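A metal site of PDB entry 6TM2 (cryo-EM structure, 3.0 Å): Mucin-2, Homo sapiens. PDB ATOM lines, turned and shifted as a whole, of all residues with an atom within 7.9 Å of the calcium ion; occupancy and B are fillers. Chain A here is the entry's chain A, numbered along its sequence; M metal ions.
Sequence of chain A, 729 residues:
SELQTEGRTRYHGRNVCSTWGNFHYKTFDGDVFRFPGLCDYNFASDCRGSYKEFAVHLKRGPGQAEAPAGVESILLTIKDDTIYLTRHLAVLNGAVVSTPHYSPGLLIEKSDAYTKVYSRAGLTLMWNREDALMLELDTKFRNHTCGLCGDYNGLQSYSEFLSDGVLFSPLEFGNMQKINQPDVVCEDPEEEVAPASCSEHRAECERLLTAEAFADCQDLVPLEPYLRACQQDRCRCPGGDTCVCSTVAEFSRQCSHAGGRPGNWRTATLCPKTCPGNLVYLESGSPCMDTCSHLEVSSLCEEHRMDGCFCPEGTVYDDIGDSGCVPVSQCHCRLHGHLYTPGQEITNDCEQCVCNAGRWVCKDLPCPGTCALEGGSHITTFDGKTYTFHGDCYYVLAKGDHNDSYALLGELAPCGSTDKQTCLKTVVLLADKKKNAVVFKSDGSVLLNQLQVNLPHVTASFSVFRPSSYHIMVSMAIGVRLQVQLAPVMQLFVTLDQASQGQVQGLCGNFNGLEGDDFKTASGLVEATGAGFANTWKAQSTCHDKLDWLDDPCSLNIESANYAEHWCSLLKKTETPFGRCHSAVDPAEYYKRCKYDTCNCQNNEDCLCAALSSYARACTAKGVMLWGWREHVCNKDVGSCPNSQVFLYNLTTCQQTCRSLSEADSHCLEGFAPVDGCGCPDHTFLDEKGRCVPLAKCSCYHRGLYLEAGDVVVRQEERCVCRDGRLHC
OD1 of Asp 151 sits close to OE2 of Glu 160 (2.6 Å).
The side-chain carboxylate (OE1) of Glu 160 lies close to the backbone NH (N) of Tyr 158 (3.3 Å).
The side-chain amide nitrogen (ND2) of Asn 153 lies within hydrogen-bond range of the side-chain carboxylate (OD2) of Asp 151, at 3.4 Å.
The side-chain amide oxygen (OD1) of Asn 153 sits close to the side-chain carboxylate (OD2) of Asp 29.
OD1 of Asp 151 lies close to OG of Ser 159, at 3.2 Å.
The backbone carbonyl oxygen (O) of Asp 29 lies close to the side-chain amide oxygen (OE1) of Gln 156, 2.9 Å away.
OD2 of Asp 29 is in hydrogen-bond range of N of Gly 154 (3.1 Å).
The backbone NH (N) of Asp 29 lies close to the side-chain hydroxyl (OG1) of Thr 27, at 3.2 Å.
Residues that only touch the calcium ion: Asp 29 (3.4 Å) and Ser 159 (3.97 Å).
Within 4 Å of the calcium ion: Asp 29, Asp 151, Asn 153, Leu 155, Ser 159 and Glu 160.
The nearest printed residue that does not touch the calcium ion is Tyr 158 (4.2 Å).
The calcium ion is bound by the side-chain carboxylate (OE2) of Glu 160 (2.3 Å), the side-chain amide oxygen (OD1) of Asn 153 (2.5 Å), the backbone carbonyl oxygen (O) of Leu 155 (2.6 Å) and the side-chain carboxylate (OE1) of Glu 160 (2.9 Å).
The calcium ion has four donor atoms within binding distance.
Slightly farther from the calcium ion lies the side-chain carboxylate (OD1) of Asp 151 (2.9 Å).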
ATOM      1  N   THR A  27     -35.864   2.091 -16.653  1.00  0.00           N
ATOM      2  CA  THR A  27     -34.751   1.721 -17.509  1.00  0.00           C
ATOM      3  C   THR A  27     -33.660   1.041 -16.691  1.00  0.00           C
ATOM      4  O   THR A  27     -33.788   0.815 -15.484  1.00  0.00           O
ATOM      5  CB  THR A  27     -34.182   2.948 -18.215  1.00  0.00           C
ATOM      6  OG1 THR A  27     -33.624   3.838 -17.242  1.00  0.00           O
ATOM      7  CG2 THR A  27     -35.278   3.684 -18.955  1.00  0.00           C
ATOM      8  N   PHE A  28     -32.548   0.720 -17.352  1.00  0.00           N
ATOM      9  CA  PHE A  28     -31.384   0.191 -16.643  1.00  0.00           C
ATOM     10  C   PHE A  28     -30.705   1.205 -15.745  1.00  0.00           C
ATOM     11  O   PHE A  28     -29.874   0.819 -14.922  1.00  0.00           O
ATOM     12  CB  PHE A  28     -30.352  -0.323 -17.632  1.00  0.00           C
ATOM     13  CG  PHE A  28     -30.740  -1.571 -18.366  1.00  0.00           C
ATOM     14  CD1 PHE A  28     -30.691  -2.794 -17.733  1.00  0.00           C
ATOM     15  CD2 PHE A  28     -31.087  -1.519 -19.697  1.00  0.00           C
ATOM     16  CE1 PHE A  28     -31.025  -3.955 -18.402  1.00  0.00           C
ATOM     17  CE2 PHE A  28     -31.419  -2.682 -20.380  1.00  0.00           C
ATOM     18  CZ  PHE A  28     -31.395  -3.888 -19.724  1.00  0.00           C
ATOM     19  N   ASP A  29     -31.030   2.485 -15.878  1.00  0.00           N
ATOM     20  CA  ASP A  29     -30.416   3.575 -15.140  1.00  0.00           C
ATOM     21  C   ASP A  29     -31.484   4.418 -14.473  1.00  0.00           C
ATOM     22  O   ASP A  29     -31.520   5.637 -14.604  1.00  0.00           O
ATOM     23  CB  ASP A  29     -29.563   4.436 -16.061  1.00  0.00           C
ATOM     24  CG  ASP A  29     -28.395   3.680 -16.633  1.00  0.00           C
ATOM     25  OD1 ASP A  29     -27.910   2.749 -15.967  1.00  0.00           O
ATOM     26  OD2 ASP A  29     -27.965   4.012 -17.753  1.00  0.00           O
ATOM     27  N   ASP A  31     -34.887   6.135 -14.310  1.00  0.00           N
ATOM     28  CA  ASP A  31     -35.770   6.720 -15.327  1.00  0.00           C
ATOM     29  C   ASP A  31     -37.136   6.041 -15.349  1.00  0.00           C
ATOM     30  O   ASP A  31     -37.512   5.359 -16.308  1.00  0.00           O
ATOM     31  CB  ASP A  31     -35.129   6.701 -16.719  1.00  0.00           C
ATOM     32  CG  ASP A  31     -33.937   7.612 -16.827  1.00  0.00           C
ATOM     33  OD1 ASP A  31     -33.912   8.626 -16.101  1.00  0.00           O
ATOM     34  OD2 ASP A  31     -33.039   7.322 -17.642  1.00  0.00           O
ATOM     35  N   ASN A 143     -22.934   0.265 -23.128  1.00  0.00           N
ATOM     36  CA  ASN A 143     -22.919   1.145 -24.296  1.00  0.00           C
ATOM     37  C   ASN A 143     -23.445   0.484 -25.570  1.00  0.00           C
ATOM     38  O   ASN A 143     -23.206   0.996 -26.664  1.00  0.00           O
ATOM     39  CB  ASN A 143     -21.517   1.717 -24.605  1.00  0.00           C
ATOM     40  CG  ASN A 143     -21.060   2.748 -23.576  1.00  0.00           C
ATOM     41  OD1 ASN A 143     -21.854   3.553 -23.100  1.00  0.00           O
ATOM     42  ND2 ASN A 143     -19.741   2.723 -23.283  1.00  0.00           N
ATOM     43  N   CYS A 149     -35.722   0.264 -22.757  1.00  0.00           N
ATOM     44  CA  CYS A 149     -35.014   0.251 -21.494  1.00  0.00           C
ATOM     45  C   CYS A 149     -33.801   1.166 -21.461  1.00  0.00           C
ATOM     46  O   CYS A 149     -32.970   1.030 -20.572  1.00  0.00           O
ATOM     47  CB  CYS A 149     -34.572  -1.174 -21.158  1.00  0.00           C
ATOM     48  SG  CYS A 149     -35.891  -2.345 -20.852  1.00  0.00           S
ATOM     49  N   GLY A 150     -33.662   2.059 -22.438  1.00  0.00           N
ATOM     50  CA  GLY A 150     -32.523   2.945 -22.507  1.00  0.00           C
ATOM     51  C   GLY A 150     -31.251   2.221 -22.901  1.00  0.00           C
ATOM     52  O   GLY A 150     -31.221   1.023 -23.174  1.00  0.00           O
ATOM     53  N   ASP A 151     -30.167   2.992 -22.944  1.00  0.00           N
ATOM     54  CA  ASP A 151     -28.853   2.399 -23.057  1.00  0.00           C
ATOM     55  C   ASP A 151     -28.307   2.060 -21.670  1.00  0.00           C
ATOM     56  O   ASP A 151     -28.903   2.392 -20.642  1.00  0.00           O
ATOM     57  CB  ASP A 151     -27.909   3.302 -23.854  1.00  0.00           C
ATOM     58  CG  ASP A 151     -27.798   4.715 -23.269  1.00  0.00           C
ATOM     59  OD1 ASP A 151     -28.518   5.043 -22.303  1.00  0.00           O
ATOM     60  OD2 ASP A 151     -26.991   5.497 -23.806  1.00  0.00           O
ATOM     61  N   TYR A 152     -27.166   1.379 -21.649  1.00  0.00           N
ATOM     62  CA  TYR A 152     -26.693   0.747 -20.427  1.00  0.00           C
ATOM     63  C   TYR A 152     -25.302   1.269 -20.120  1.00  0.00           C
ATOM     64  O   TYR A 152     -24.356   0.519 -19.893  1.00  0.00           O
ATOM     65  CB  TYR A 152     -26.791  -0.779 -20.599  1.00  0.00           C
ATOM     66  CG  TYR A 152     -26.431  -1.657 -19.426  1.00  0.00           C
ATOM     67  CD1 TYR A 152     -27.165  -1.610 -18.255  1.00  0.00           C
ATOM     68  CD2 TYR A 152     -25.469  -2.646 -19.540  1.00  0.00           C
ATOM     69  CE1 TYR A 152     -26.879  -2.417 -17.184  1.00  0.00           C
ATOM     70  CE2 TYR A 152     -25.178  -3.483 -18.478  1.00  0.00           C
ATOM     71  CZ  TYR A 152     -25.888  -3.356 -17.310  1.00  0.00           C
ATOM     72  OH  TYR A 152     -25.621  -4.179 -16.240  1.00  0.00           O
ATOM     73  N   ASN A 153     -25.182   2.598 -20.136  1.00  0.00           N
ATOM     74  CA  ASN A 153     -23.958   3.316 -19.837  1.00  0.00           C
ATOM     75  C   ASN A 153     -23.775   3.639 -18.362  1.00  0.00           C
ATOM     76  O   ASN A 153     -22.641   3.888 -17.926  1.00  0.00           O
ATOM     77  CB  ASN A 153     -23.904   4.611 -20.669  1.00  0.00           C
ATOM     78  CG  ASN A 153     -25.111   5.535 -20.436  1.00  0.00           C
ATOM     79  OD1 ASN A 153     -25.966   5.279 -19.589  1.00  0.00           O
ATOM     80  ND2 ASN A 153     -25.169   6.618 -21.206  1.00  0.00           N
ATOM     81  N   GLY A 154     -24.856   3.632 -17.577  1.00  0.00           N
ATOM     82  CA  GLY A 154     -24.785   3.977 -16.181  1.00  0.00           C
ATOM     83  C   GLY A 154     -25.167   5.407 -15.855  1.00  0.00           C
ATOM     84  O   GLY A 154     -25.259   5.747 -14.672  1.00  0.00           O
ATOM     85  N   LEU A 155     -25.413   6.236 -16.858  1.00  0.00           N
ATOM     86  CA  LEU A 155     -25.677   7.653 -16.643  1.00  0.00           C
ATOM     87  C   LEU A 155     -27.190   7.892 -16.552  1.00  0.00           C
ATOM     88  O   LEU A 155     -27.933   7.518 -17.466  1.00  0.00           O
ATOM     89  CB  LEU A 155     -25.068   8.486 -17.762  1.00  0.00           C
ATOM     90  N   GLN A 156     -27.619   8.513 -15.453  1.00  0.00           N
ATOM     91  CA  GLN A 156     -29.010   8.852 -15.208  1.00  0.00           C
ATOM     92  C   GLN A 156     -29.535   9.870 -16.220  1.00  0.00           C
ATOM     93  O   GLN A 156     -29.120  11.027 -16.212  1.00  0.00           O
ATOM     94  CB  GLN A 156     -29.163   9.435 -13.806  1.00  0.00           C
ATOM     95  CG  GLN A 156     -30.579   9.807 -13.404  1.00  0.00           C
ATOM     96  CD  GLN A 156     -31.448   8.600 -13.175  1.00  0.00           C
ATOM     97  OE1 GLN A 156     -31.023   7.620 -12.561  1.00  0.00           O
ATOM     98  NE2 GLN A 156     -32.686   8.663 -13.643  1.00  0.00           N
ATOM     99  N   SER A 157     -30.449   9.428 -17.098  1.00  0.00           N
ATOM    100  CA  SER A 157     -31.225  10.266 -18.024  1.00  0.00           C
ATOM    101  C   SER A 157     -30.362  11.078 -18.978  1.00  0.00           C
ATOM    102  O   SER A 157     -30.799  12.122 -19.474  1.00  0.00           O
ATOM    103  CB  SER A 157     -32.171  11.199 -17.259  1.00  0.00           C
ATOM    104  OG  SER A 157     -32.888  12.030 -18.161  1.00  0.00           O
ATOM    105  N   TYR A 158     -29.136  10.626 -19.280  1.00  0.00           N
ATOM    106  CA  TYR A 158     -28.228  11.451 -20.063  1.00  0.00           C
ATOM    107  C   TYR A 158     -28.541  11.362 -21.553  1.00  0.00           C
ATOM    108  O   TYR A 158     -28.946  12.349 -22.172  1.00  0.00           O
ATOM    109  CB  TYR A 158     -26.780  11.034 -19.793  1.00  0.00           C
ATOM    110  N   SER A 159     -28.378  10.182 -22.135  1.00  0.00           N
ATOM    111  CA  SER A 159     -28.538  10.017 -23.582  1.00  0.00           C
ATOM    112  C   SER A 159     -29.883   9.439 -23.974  1.00  0.00           C
ATOM    113  O   SER A 159     -30.152   9.312 -25.168  1.00  0.00           O
ATOM    114  CB  SER A 159     -27.412   9.126 -24.131  1.00  0.00           C
ATOM    115  OG  SER A 159     -27.513   7.817 -23.608  1.00  0.00           O
ATOM    116  N   GLU A 160     -30.735   9.082 -23.015  1.00  0.00           N
ATOM    117  CA  GLU A 160     -32.064   8.594 -23.354  1.00  0.00           C
ATOM    118  C   GLU A 160     -32.980   9.734 -23.743  1.00  0.00           C
ATOM    119  O   GLU A 160     -33.663   9.675 -24.773  1.00  0.00           O
ATOM    120  CB  GLU A 160     -32.675   7.813 -22.185  1.00  0.00           C
ATOM    121  CG  GLU A 160     -31.967   6.521 -21.810  1.00  0.00           C
ATOM    122  CD  GLU A 160     -30.849   6.733 -20.797  1.00  0.00           C
ATOM    123  OE1 GLU A 160     -30.654   7.887 -20.366  1.00  0.00           O
ATOM    124  OE2 GLU A 160     -30.187   5.740 -20.421  1.00  0.00           O
ATOM    125  N   PHE A 161     -33.012  10.790 -22.932  1.00  0.00           N
ATOM    126  CA  PHE A 161     -33.962  11.878 -23.114  1.00  0.00           C
ATOM    127  C   PHE A 161     -33.346  13.148 -23.675  1.00  0.00           C
ATOM    128  O   PHE A 161     -34.071  13.945 -24.282  1.00  0.00           O
ATOM    129  CB  PHE A 161     -34.652  12.215 -21.783  1.00  0.00           C
ATOM    130  CG  PHE A 161     -35.601  11.151 -21.286  1.00  0.00           C
ATOM    131  CD1 PHE A 161     -36.067  10.152 -22.132  1.00  0.00           C
ATOM    132  CD2 PHE A 161     -36.048  11.161 -19.971  1.00  0.00           C
ATOM    133  CE1 PHE A 161     -36.938   9.193 -21.677  1.00  0.00           C
ATOM    134  CE2 PHE A 161     -36.920  10.202 -19.516  1.00  0.00           C
ATOM    135  CZ  PHE A 161     -37.364   9.211 -20.367  1.00  0.00           C
HETATM  136 CA    CA M   1     -28.109   6.614 -19.872  1.00  0.00          CA
